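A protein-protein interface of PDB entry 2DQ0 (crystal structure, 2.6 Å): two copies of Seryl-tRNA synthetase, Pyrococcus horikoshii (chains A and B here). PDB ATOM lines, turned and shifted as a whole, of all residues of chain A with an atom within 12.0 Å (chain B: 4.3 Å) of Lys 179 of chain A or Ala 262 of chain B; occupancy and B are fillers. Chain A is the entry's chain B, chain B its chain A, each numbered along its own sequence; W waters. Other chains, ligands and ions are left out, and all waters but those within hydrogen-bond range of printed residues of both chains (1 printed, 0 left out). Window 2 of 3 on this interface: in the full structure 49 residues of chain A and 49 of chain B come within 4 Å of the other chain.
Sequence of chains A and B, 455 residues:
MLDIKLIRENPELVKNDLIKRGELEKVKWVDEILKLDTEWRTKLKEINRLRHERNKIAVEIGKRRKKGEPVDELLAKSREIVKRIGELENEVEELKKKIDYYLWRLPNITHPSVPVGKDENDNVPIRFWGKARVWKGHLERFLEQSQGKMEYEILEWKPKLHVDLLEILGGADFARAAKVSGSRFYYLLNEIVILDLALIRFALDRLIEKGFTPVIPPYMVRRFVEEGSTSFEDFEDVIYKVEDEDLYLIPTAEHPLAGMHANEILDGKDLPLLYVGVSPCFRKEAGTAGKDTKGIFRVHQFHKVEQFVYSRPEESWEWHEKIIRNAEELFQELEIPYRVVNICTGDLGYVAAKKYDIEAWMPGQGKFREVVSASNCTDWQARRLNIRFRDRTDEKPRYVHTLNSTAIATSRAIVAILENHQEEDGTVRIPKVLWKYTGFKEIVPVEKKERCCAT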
ATOM      1  N   ALA A 172       0.356  33.910 -13.312  1.00  0.00           N
ATOM      2  CA  ALA A 172       0.340  32.517 -12.877  1.00  0.00           C
ATOM      3  C   ALA A 172       0.323  32.372 -11.356  1.00  0.00           C
ATOM      4  O   ALA A 172       0.679  33.299 -10.637  1.00  0.00           O
ATOM      5  CB  ALA A 172       1.568  31.776 -13.456  1.00  0.00           C
ATOM      6  N   ASP A 173      -0.134  31.218 -10.880  1.00  0.00           N
ATOM      7  CA  ASP A 173      -0.132  30.912  -9.457  1.00  0.00           C
ATOM      8  C   ASP A 173       0.294  29.443  -9.384  1.00  0.00           C
ATOM      9  O   ASP A 173      -0.459  28.557  -9.793  1.00  0.00           O
ATOM     10  CB  ASP A 173      -1.521  31.083  -8.823  1.00  0.00           C
ATOM     11  CG  ASP A 173      -1.520  30.864  -7.280  1.00  0.00           C
ATOM     12  OD1 ASP A 173      -0.890  29.898  -6.776  1.00  0.00           O
ATOM     13  OD2 ASP A 173      -2.182  31.652  -6.569  1.00  0.00           O
ATOM     14  N   PHE A 174       1.503  29.192  -8.880  1.00  0.00           N
ATOM     15  CA  PHE A 174       1.994  27.834  -8.776  1.00  0.00           C
ATOM     16  C   PHE A 174       1.700  27.174  -7.443  1.00  0.00           C
ATOM     17  O   PHE A 174       1.347  25.997  -7.388  1.00  0.00           O
ATOM     18  CB  PHE A 174       3.494  27.791  -9.050  1.00  0.00           C
ATOM     19  CG  PHE A 174       3.858  28.121 -10.468  1.00  0.00           C
ATOM     20  CD1 PHE A 174       4.303  29.405 -10.809  1.00  0.00           C
ATOM     21  CD2 PHE A 174       3.754  27.145 -11.471  1.00  0.00           C
ATOM     22  CE1 PHE A 174       4.642  29.713 -12.120  1.00  0.00           C
ATOM     23  CE2 PHE A 174       4.091  27.434 -12.799  1.00  0.00           C
ATOM     24  CZ  PHE A 174       4.538  28.726 -13.126  1.00  0.00           C
ATOM     25  N   ALA A 175       1.844  27.929  -6.364  1.00  0.00           N
ATOM     26  CA  ALA A 175       1.596  27.383  -5.030  1.00  0.00           C
ATOM     27  C   ALA A 175       0.203  26.782  -4.928  1.00  0.00           C
ATOM     28  O   ALA A 175       0.044  25.623  -4.519  1.00  0.00           O
ATOM     29  CB  ALA A 175       1.770  28.467  -3.977  1.00  0.00           C
ATOM     30  N   ARG A 176      -0.814  27.553  -5.296  1.00  0.00           N
ATOM     31  CA  ARG A 176      -2.147  26.992  -5.202  1.00  0.00           C
ATOM     32  C   ARG A 176      -2.364  25.760  -6.107  1.00  0.00           C
ATOM     33  O   ARG A 176      -3.113  24.841  -5.759  1.00  0.00           O
ATOM     34  CB  ARG A 176      -3.179  28.076  -5.445  1.00  0.00           C
ATOM     35  CG  ARG A 176      -3.227  29.040  -4.290  1.00  0.00           C
ATOM     36  CD  ARG A 176      -4.331  30.038  -4.471  1.00  0.00           C
ATOM     37  NE  ARG A 176      -4.499  30.867  -3.290  1.00  0.00           N
ATOM     38  CZ  ARG A 176      -3.853  32.008  -3.076  1.00  0.00           C
ATOM     39  NH1 ARG A 176      -4.083  32.691  -1.961  1.00  0.00           N
ATOM     40  NH2 ARG A 176      -2.989  32.476  -3.976  1.00  0.00           N
ATOM     41  N   ALA A 177      -1.680  25.722  -7.242  1.00  0.00           N
ATOM     42  CA  ALA A 177      -1.801  24.580  -8.131  1.00  0.00           C
ATOM     43  C   ALA A 177      -1.212  23.340  -7.462  1.00  0.00           C
ATOM     44  O   ALA A 177      -1.727  22.234  -7.602  1.00  0.00           O
ATOM     45  CB  ALA A 177      -1.090  24.864  -9.412  1.00  0.00           C
ATOM     46  N   ALA A 178      -0.119  23.527  -6.733  1.00  0.00           N
ATOM     47  CA  ALA A 178       0.524  22.417  -6.045  1.00  0.00           C
ATOM     48  C   ALA A 178      -0.395  21.910  -4.960  1.00  0.00           C
ATOM     49  O   ALA A 178      -0.439  20.719  -4.668  1.00  0.00           O
ATOM     50  CB  ALA A 178       1.818  22.868  -5.440  1.00  0.00           C
ATOM     51  N   LYS A 179      -1.146  22.821  -4.368  1.00  0.00           N
ATOM     52  CA  LYS A 179      -2.047  22.438  -3.303  1.00  0.00           C
ATOM     53  C   LYS A 179      -3.123  21.504  -3.814  1.00  0.00           C
ATOM     54  O   LYS A 179      -3.334  20.417  -3.295  1.00  0.00           O
ATOM     55  CB  LYS A 179      -2.696  23.693  -2.688  1.00  0.00           C
ATOM     56  CG  LYS A 179      -3.807  23.397  -1.680  1.00  0.00           C
ATOM     57  CD  LYS A 179      -4.399  24.666  -1.075  1.00  0.00           C
ATOM     58  CE  LYS A 179      -4.794  25.690  -2.121  1.00  0.00           C
ATOM     59  NZ  LYS A 179      -5.226  26.980  -1.485  1.00  0.00           N
ATOM     60  N   VAL A 180      -3.769  21.952  -4.875  1.00  0.00           N
ATOM     61  CA  VAL A 180      -4.880  21.276  -5.485  1.00  0.00           C
ATOM     62  C   VAL A 180      -4.576  20.081  -6.402  1.00  0.00           C
ATOM     63  O   VAL A 180      -5.420  19.187  -6.552  1.00  0.00           O
ATOM     64  CB  VAL A 180      -5.693  22.323  -6.263  1.00  0.00           C
ATOM     65  CG1 VAL A 180      -5.190  22.418  -7.671  1.00  0.00           C
ATOM     66  CG2 VAL A 180      -7.116  21.995  -6.243  1.00  0.00           C
ATOM     67  N   SER A 181      -3.389  20.044  -7.002  1.00  0.00           N
ATOM     68  CA  SER A 181      -3.072  18.971  -7.946  1.00  0.00           C
ATOM     69  C   SER A 181      -1.722  18.300  -7.760  1.00  0.00           C
ATOM     70  O   SER A 181      -1.548  17.135  -8.087  1.00  0.00           O
ATOM     71  CB  SER A 181      -3.143  19.497  -9.399  1.00  0.00           C
ATOM     72  OG  SER A 181      -4.372  20.143  -9.674  1.00  0.00           O
ATOM     73  N   GLY A 182      -0.759  19.033  -7.237  1.00  0.00           N
ATOM     74  CA  GLY A 182       0.552  18.452  -7.073  1.00  0.00           C
ATOM     75  C   GLY A 182       1.514  19.326  -7.840  1.00  0.00           C
ATOM     76  O   GLY A 182       1.114  20.320  -8.459  1.00  0.00           O
ATOM     77  N   SER A 183       2.788  18.970  -7.825  1.00  0.00           N
ATOM     78  CA  SER A 183       3.751  19.804  -8.515  1.00  0.00           C
ATOM     79  C   SER A 183       3.663  19.704 -10.037  1.00  0.00           C
ATOM     80  O   SER A 183       3.061  18.790 -10.597  1.00  0.00           O
ATOM     81  CB  SER A 183       5.158  19.472  -8.043  1.00  0.00           C
ATOM     82  OG  SER A 183       5.472  18.131  -8.351  1.00  0.00           O
ATOM     83  N   ARG A 184       4.297  20.665 -10.685  1.00  0.00           N
ATOM     84  CA  ARG A 184       4.334  20.772 -12.117  1.00  0.00           C
ATOM     85  C   ARG A 184       2.951  20.897 -12.771  1.00  0.00           C
ATOM     86  O   ARG A 184       2.710  20.412 -13.870  1.00  0.00           O
ATOM     87  CB  ARG A 184       5.198  19.648 -12.716  1.00  0.00           C
ATOM     88  CG  ARG A 184       6.693  19.791 -12.304  1.00  0.00           C
ATOM     89  CD  ARG A 184       7.710  18.954 -13.136  1.00  0.00           C
ATOM     90  NE  ARG A 184       7.520  17.509 -13.010  1.00  0.00           N
ATOM     91  CZ  ARG A 184       8.195  16.602 -13.712  1.00  0.00           C
ATOM     92  NH1 ARG A 184       7.950  15.296 -13.534  1.00  0.00           N
ATOM     93  NH2 ARG A 184       9.114  17.004 -14.597  1.00  0.00           N
ATOM     94  N   PHE A 185       2.061  21.577 -12.053  1.00  0.00           N
ATOM     95  CA  PHE A 185       0.710  21.923 -12.489  1.00  0.00           C
ATOM     96  C   PHE A 185       0.674  23.421 -12.186  1.00  0.00           C
ATOM     97  O   PHE A 185       1.541  23.931 -11.458  1.00  0.00           O
ATOM     98  CB  PHE A 185      -0.375  21.201 -11.676  1.00  0.00           C
ATOM     99  CG  PHE A 185      -0.775  19.860 -12.245  1.00  0.00           C
ATOM    100  CD1 PHE A 185      -0.397  18.679 -11.613  1.00  0.00           C
ATOM    101  CD2 PHE A 185      -1.516  19.784 -13.428  1.00  0.00           C
ATOM    102  CE1 PHE A 185      -0.752  17.437 -12.150  1.00  0.00           C
ATOM    103  CE2 PHE A 185      -1.872  18.560 -13.971  1.00  0.00           C
ATOM    104  CZ  PHE A 185      -1.490  17.373 -13.330  1.00  0.00           C
ATOM    105  N   TYR A 186      -0.306  24.135 -12.718  1.00  0.00           N
ATOM    106  CA  TYR A 186      -0.344  25.566 -12.484  1.00  0.00           C
ATOM    107  C   TYR A 186      -1.688  26.167 -12.801  1.00  0.00           C
ATOM    108  O   TYR A 186      -2.539  25.502 -13.354  1.00  0.00           O
ATOM    109  CB  TYR A 186       0.656  26.244 -13.391  1.00  0.00           C
ATOM    110  CG  TYR A 186       0.400  25.888 -14.830  1.00  0.00           C
ATOM    111  CD1 TYR A 186       1.032  24.789 -15.403  1.00  0.00           C
ATOM    112  CD2 TYR A 186      -0.566  26.566 -15.588  1.00  0.00           C
ATOM    113  CE1 TYR A 186       0.712  24.359 -16.682  1.00  0.00           C
ATOM    114  CE2 TYR A 186      -0.897  26.136 -16.881  1.00  0.00           C
ATOM    115  CZ  TYR A 186      -0.251  25.023 -17.413  1.00  0.00           C
ATOM    116  OH  TYR A 186      -0.589  24.507 -18.637  1.00  0.00           O
ATOM    117  N   TYR A 187      -1.859  27.434 -12.432  1.00  0.00           N
ATOM    118  CA  TYR A 187      -3.051  28.185 -12.794  1.00  0.00           C
ATOM    119  C   TYR A 187      -2.442  29.315 -13.597  1.00  0.00           C
ATOM    120  O   TYR A 187      -1.486  29.937 -13.148  1.00  0.00           O
ATOM    121  CB  TYR A 187      -3.784  28.820 -11.611  1.00  0.00           C
ATOM    122  CG  TYR A 187      -4.592  27.889 -10.730  1.00  0.00           C
ATOM    123  CD1 TYR A 187      -3.965  27.092  -9.784  1.00  0.00           C
ATOM    124  CD2 TYR A 187      -5.991  27.864 -10.794  1.00  0.00           C
ATOM    125  CE1 TYR A 187      -4.693  26.297  -8.917  1.00  0.00           C
ATOM    126  CE2 TYR A 187      -6.740  27.063  -9.922  1.00  0.00           C
ATOM    127  CZ  TYR A 187      -6.068  26.282  -8.985  1.00  0.00           C
ATOM    128  OH  TYR A 187      -6.742  25.474  -8.113  1.00  0.00           O
ATOM    129  N   LYS A 294      11.469  25.778 -13.291  1.00  0.00           N
ATOM    130  CA  LYS A 294      10.274  25.507 -12.472  1.00  0.00           C
ATOM    131  C   LYS A 294       8.956  26.258 -12.733  1.00  0.00           C
ATOM    132  O   LYS A 294       8.137  26.404 -11.817  1.00  0.00           O
ATOM    133  CB  LYS A 294      10.637  25.632 -10.974  1.00  0.00           C
ATOM    134  CG  LYS A 294      11.632  24.571 -10.454  1.00  0.00           C
ATOM    135  CD  LYS A 294      11.032  23.158 -10.434  1.00  0.00           C
ATOM    136  CE  LYS A 294      10.427  22.825  -9.083  1.00  0.00           C
ATOM    137  NZ  LYS A 294       9.683  21.534  -9.126  1.00  0.00           N
ATOM    138  N   HIS A 300       2.905  18.959 -16.621  1.00  0.00           N
ATOM    139  CA  HIS A 300       2.070  17.787 -16.893  1.00  0.00           C
ATOM    140  C   HIS A 300       0.959  18.091 -17.854  1.00  0.00           C
ATOM    141  O   HIS A 300       0.334  17.167 -18.408  1.00  0.00           O
ATOM    142  CB  HIS A 300       1.394  17.287 -15.613  1.00  0.00           C
ATOM    143  CG  HIS A 300       2.348  16.756 -14.601  1.00  0.00           C
ATOM    144  ND1 HIS A 300       3.179  15.686 -14.857  1.00  0.00           N
ATOM    145  CD2 HIS A 300       2.632  17.166 -13.343  1.00  0.00           C
ATOM    146  CE1 HIS A 300       3.936  15.462 -13.800  1.00  0.00           C
ATOM    147  NE2 HIS A 300       3.624  16.347 -12.869  1.00  0.00           N
ATOM    148  N   ARG B 222      -6.485  16.737  -7.317  1.00  0.00           N
ATOM    149  CA  ARG B 222      -6.409  15.776  -6.216  1.00  0.00           C
ATOM    150  C   ARG B 222      -7.819  15.429  -5.700  1.00  0.00           C
ATOM    151  O   ARG B 222      -8.718  16.264  -5.714  1.00  0.00           O
ATOM    152  CB  ARG B 222      -5.573  16.404  -5.105  1.00  0.00           C
ATOM    153  CG  ARG B 222      -4.872  15.434  -4.221  1.00  0.00           C
ATOM    154  CD  ARG B 222      -3.380  15.491  -4.427  1.00  0.00           C
ATOM    155  NE  ARG B 222      -2.853  16.816  -4.129  1.00  0.00           N
ATOM    156  CZ  ARG B 222      -1.557  17.101  -4.041  1.00  0.00           C
ATOM    157  NH1 ARG B 222      -1.179  18.342  -3.768  1.00  0.00           N
ATOM    158  NH2 ARG B 222      -0.641  16.149  -4.221  1.00  0.00           N
ATOM    159  N   PHE B 224      -9.361  15.370  -2.884  1.00  0.00           N
ATOM    160  CA  PHE B 224     -10.024  16.253  -1.930  1.00  0.00           C
ATOM    161  C   PHE B 224     -10.719  17.441  -2.575  1.00  0.00           C
ATOM    162  O   PHE B 224     -11.761  17.858  -2.098  1.00  0.00           O
ATOM    163  CB  PHE B 224      -9.045  16.718  -0.839  1.00  0.00           C
ATOM    164  CG  PHE B 224      -8.248  17.910  -1.210  1.00  0.00           C
ATOM    165  CD1 PHE B 224      -8.669  19.179  -0.831  1.00  0.00           C
ATOM    166  CD2 PHE B 224      -7.045  17.771  -1.906  1.00  0.00           C
ATOM    167  CE1 PHE B 224      -7.906  20.314  -1.126  1.00  0.00           C
ATOM    168  CE2 PHE B 224      -6.275  18.893  -2.207  1.00  0.00           C
ATOM    169  CZ  PHE B 224      -6.707  20.176  -1.810  1.00  0.00           C
ATOM    170  N   ALA B 258     -12.711  26.184  -7.200  1.00  0.00           N
ATOM    171  CA  ALA B 258     -13.088  26.204  -5.789  1.00  0.00           C
ATOM    172  C   ALA B 258     -11.930  25.695  -4.920  1.00  0.00           C
ATOM    173  O   ALA B 258     -11.667  26.228  -3.846  1.00  0.00           O
ATOM    174  CB  ALA B 258     -14.336  25.358  -5.551  1.00  0.00           C
ATOM    175  N   GLY B 259     -11.230  24.669  -5.375  1.00  0.00           N
ATOM    176  CA  GLY B 259     -10.123  24.181  -4.585  1.00  0.00           C
ATOM    177  C   GLY B 259      -8.995  25.202  -4.525  1.00  0.00           C
ATOM    178  O   GLY B 259      -8.162  25.157  -3.621  1.00  0.00           O
ATOM    179  N   MET B 260      -8.970  26.127  -5.479  1.00  0.00           N
ATOM    180  CA  MET B 260      -7.929  27.156  -5.544  1.00  0.00           C
ATOM    181  C   MET B 260      -7.605  27.852  -4.213  1.00  0.00           C
ATOM    182  O   MET B 260      -6.454  28.171  -3.940  1.00  0.00           O
ATOM    183  CB  MET B 260      -8.305  28.213  -6.593  1.00  0.00           C
ATOM    184  CG  MET B 260      -7.322  29.373  -6.718  1.00  0.00           C
ATOM    185  SD  MET B 260      -7.842  30.605  -7.956  1.00  0.00           S
ATOM    186  CE  MET B 260      -6.457  30.597  -9.012  1.00  0.00           C
ATOM    187  N   HIS B 261      -8.621  28.098  -3.394  1.00  0.00           N
ATOM    188  CA  HIS B 261      -8.413  28.759  -2.115  1.00  0.00           C
ATOM    189  C   HIS B 261      -8.756  27.869  -0.924  1.00  0.00           C
ATOM    190  O   HIS B 261      -9.115  28.359   0.142  1.00  0.00           O
ATOM    191  CB  HIS B 261      -9.232  30.051  -2.051  1.00  0.00           C
ATOM    192  CG  HIS B 261      -8.748  31.118  -2.980  1.00  0.00           C
ATOM    193  ND1 HIS B 261      -7.523  31.736  -2.829  1.00  0.00           N
ATOM    194  CD2 HIS B 261      -9.323  31.681  -4.070  1.00  0.00           C
ATOM    195  CE1 HIS B 261      -7.365  32.635  -3.787  1.00  0.00           C
ATOM    196  NE2 HIS B 261      -8.443  32.621  -4.553  1.00  0.00           N
ATOM    197  N   ALA B 262      -8.661  26.558  -1.116  1.00  0.00           N
ATOM    198  CA  ALA B 262      -8.936  25.610  -0.041  1.00  0.00           C
ATOM    199  C   ALA B 262      -7.970  25.913   1.103  1.00  0.00           C
ATOM    200  O   ALA B 262      -6.801  26.200   0.862  1.00  0.00           O
ATOM    201  CB  ALA B 262      -8.722  24.168  -0.529  1.00  0.00           C
ATOM    202  N   ASN B 263      -8.473  25.852   2.334  1.00  0.00           N
ATOM    203  CA  ASN B 263      -7.692  26.100   3.545  1.00  0.00           C
ATOM    204  C   ASN B 263      -7.111  27.514   3.622  1.00  0.00           C
ATOM    205  O   ASN B 263      -5.930  27.697   3.877  1.00  0.00           O
ATOM    206  CB  ASN B 263      -6.564  25.066   3.671  1.00  0.00           C
ATOM    207  CG  ASN B 263      -7.080  23.662   3.925  1.00  0.00           C
ATOM    208  OD1 ASN B 263      -6.536  22.686   3.403  1.00  0.00           O
ATOM    209  ND2 ASN B 263      -8.127  23.547   4.738  1.00  0.00           N
ATOM    210  N   GLU B 264      -7.937  28.517   3.377  1.00  0.00           N
ATOM    211  CA  GLU B 264      -7.472  29.889   3.461  1.00  0.00           C
ATOM    212  C   GLU B 264      -8.476  30.684   4.254  1.00  0.00           C
ATOM    213  O   GLU B 264      -9.653  30.321   4.351  1.00  0.00           O
ATOM    214  CB  GLU B 264      -7.348  30.557   2.080  1.00  0.00           C
ATOM    215  CG  GLU B 264      -6.335  29.938   1.125  1.00  0.00           C
ATOM    216  CD  GLU B 264      -6.136  30.772  -0.135  1.00  0.00           C
ATOM    217  OE1 GLU B 264      -5.591  30.246  -1.125  1.00  0.00           O
ATOM    218  OE2 GLU B 264      -6.515  31.963  -0.138  1.00  0.00           O
ATOM    219  N   LEU B 385     -14.067  22.656   1.912  1.00  0.00           N
ATOM    220  CA  LEU B 385     -12.717  23.046   1.543  1.00  0.00           C
ATOM    221  C   LEU B 385     -12.057  23.987   2.548  1.00  0.00           C
ATOM    222  O   LEU B 385     -10.920  24.414   2.350  1.00  0.00           O
ATOM    223  CB  LEU B 385     -12.750  23.691   0.162  1.00  0.00           C
ATOM    224  CG  LEU B 385     -13.299  22.726  -0.885  1.00  0.00           C
ATOM    225  CD1 LEU B 385     -13.515  23.442  -2.223  1.00  0.00           C
ATOM    226  CD2 LEU B 385     -12.326  21.556  -1.005  1.00  0.00           C
ATOM    227  N   ILE B 387     -12.890  27.209   3.483  1.00  0.00           N
ATOM    228  CA  ILE B 387     -12.647  28.510   2.904  1.00  0.00           C
ATOM    229  C   ILE B 387     -13.411  29.543   3.706  1.00  0.00           C
ATOM    230  O   ILE B 387     -14.627  29.705   3.558  1.00  0.00           O
ATOM    231  CB  ILE B 387     -13.089  28.549   1.445  1.00  0.00           C
ATOM    232  CG1 ILE B 387     -12.281  27.529   0.648  1.00  0.00           C
ATOM    233  CG2 ILE B 387     -12.888  29.935   0.875  1.00  0.00           C
ATOM    234  CD1 ILE B 387     -12.660  27.488  -0.795  1.00  0.00           C
HETATM  235  O   HOH W   1      -1.650  14.404  -6.856  1.00  0.00           O
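Arg 222 of chain B touches just these residues of chain A: Ala 178, Lys 179, Val 180, Ser 181 and Gly 182.
No residue of chain A comes within 4 Å of Ala 258 of chain B.
No residue of chain A comes within 4 Å of Asn 263 of chain B.
No residue of chain A comes within 4 Å of Leu 385 of chain B.
No residue of chain A comes within 4 Å of Ile 387 of chain B.
Of the printed residues of chain B, Ser 181 of chain A touches Arg 222.
Printed residues of chain B within 4 Å of Arg 176 of chain A: Met 260, His 261 and Glu 264.
Of the printed residues of chain B, Gly 182 of chain A touches Arg 222 (3.6 Å).
The nearest printed residue of chain A that does not touch Met 260 of chain B is Val 180 of chain A (4.6 Å).
Among the printed residues, merely in contact across the chains: Lys 179 of chain A with Phe 224 of chain B (3.5 Å), Lys 179 of chain A with Gly 259 of chain B (3.7 Å), Lys 179 of chain A with His 261 of chain B (3.7 Å), Ser 181 of chain A with Arg 222 of chain B (3.9 Å), Gly 182 of chain A with Arg 222 of chain B (3.6 Å) and Tyr 187 of chain A with Met 260 of chain B (3.3 Å).
N of Asp 173 of chain A is in hydrogen-bond range of O of Tyr 187 of chain A, 2.9 Å away.
The backbone carbonyl oxygen (O) of Ala 177 of chain A sits at hydrogen-bond distance from the backbone NH (N) of Gly 182 of chain A, at 3.4 Å.
OE2 of Glu 264 of chain B lies within hydrogen-bond range of ND1 of His 261 of chain B (2.9 Å).
The side-chain carboxylate (OD2) of Asp 173 of chain A is in salt-bridge range of the guanidinium group (NH2) of Arg 176 of chain A.
Hydrophobic or aromatic side chains of chain A within 4 Å of the printed part of chain B: Tyr 187.
Along chain A the printed residues that touch a printed residue of chain B span positions 176 to 187.
Hydrophobic or aromatic side chains of chain B within 4 Å of the printed part of chain A: Phe 224, Met 260 and His 261.
Water W1 lies within hydrogen-bond range of the backbone carbonyl oxygen (O) of Ser 181 of chain A and the guanidinium group (NH2) of Arg 222 of chain B.
No position is printed for both chains.
The backbone carbonyl oxygen of Met 260 of chain B lies close to the guanidinium group of Arg 176 of chain A.
NH1 of Arg 222 of chain B is in hydrogen-bond range of O of Lys 179 of chain A, at 3.0 Å.
The side-chain amino group of Lys 179 of chain A sits at hydrogen-bond distance from the backbone carbonyl oxygen of Ala 262 of chain B (2.9 Å).
OE1 of Glu 264 of chain B is in salt-bridge range of NZ of Lys 179 of chain A (3.3 Å).
The backbone carbonyl oxygen of Met 260 of chain B lies within hydrogen-bond range of the side-chain amino group of Lys 179 of chain A (3.0 Å).
A ring nitrogen (ND1) of His 261 of chain B lies within hydrogen-bond range of the guanidinium group (NE) of Arg 176 of chain A (3.2 Å).
The side-chain carboxylate (OE1) of Glu 264 of chain B lies within salt-bridge range of the guanidinium group (NE) of Arg 176 of chain A (2.5 Å).
The backbone carbonyl oxygen (O) of Ala 178 of chain A sits at hydrogen-bond distance from the guanidinium group (NH1) of Arg 222 of chain B, 2.6 Å away.
The backbone carbonyl oxygen (O) of Val 180 of chain A lies within hydrogen-bond range of the backbone NH (N) of Arg 222 of chain B.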
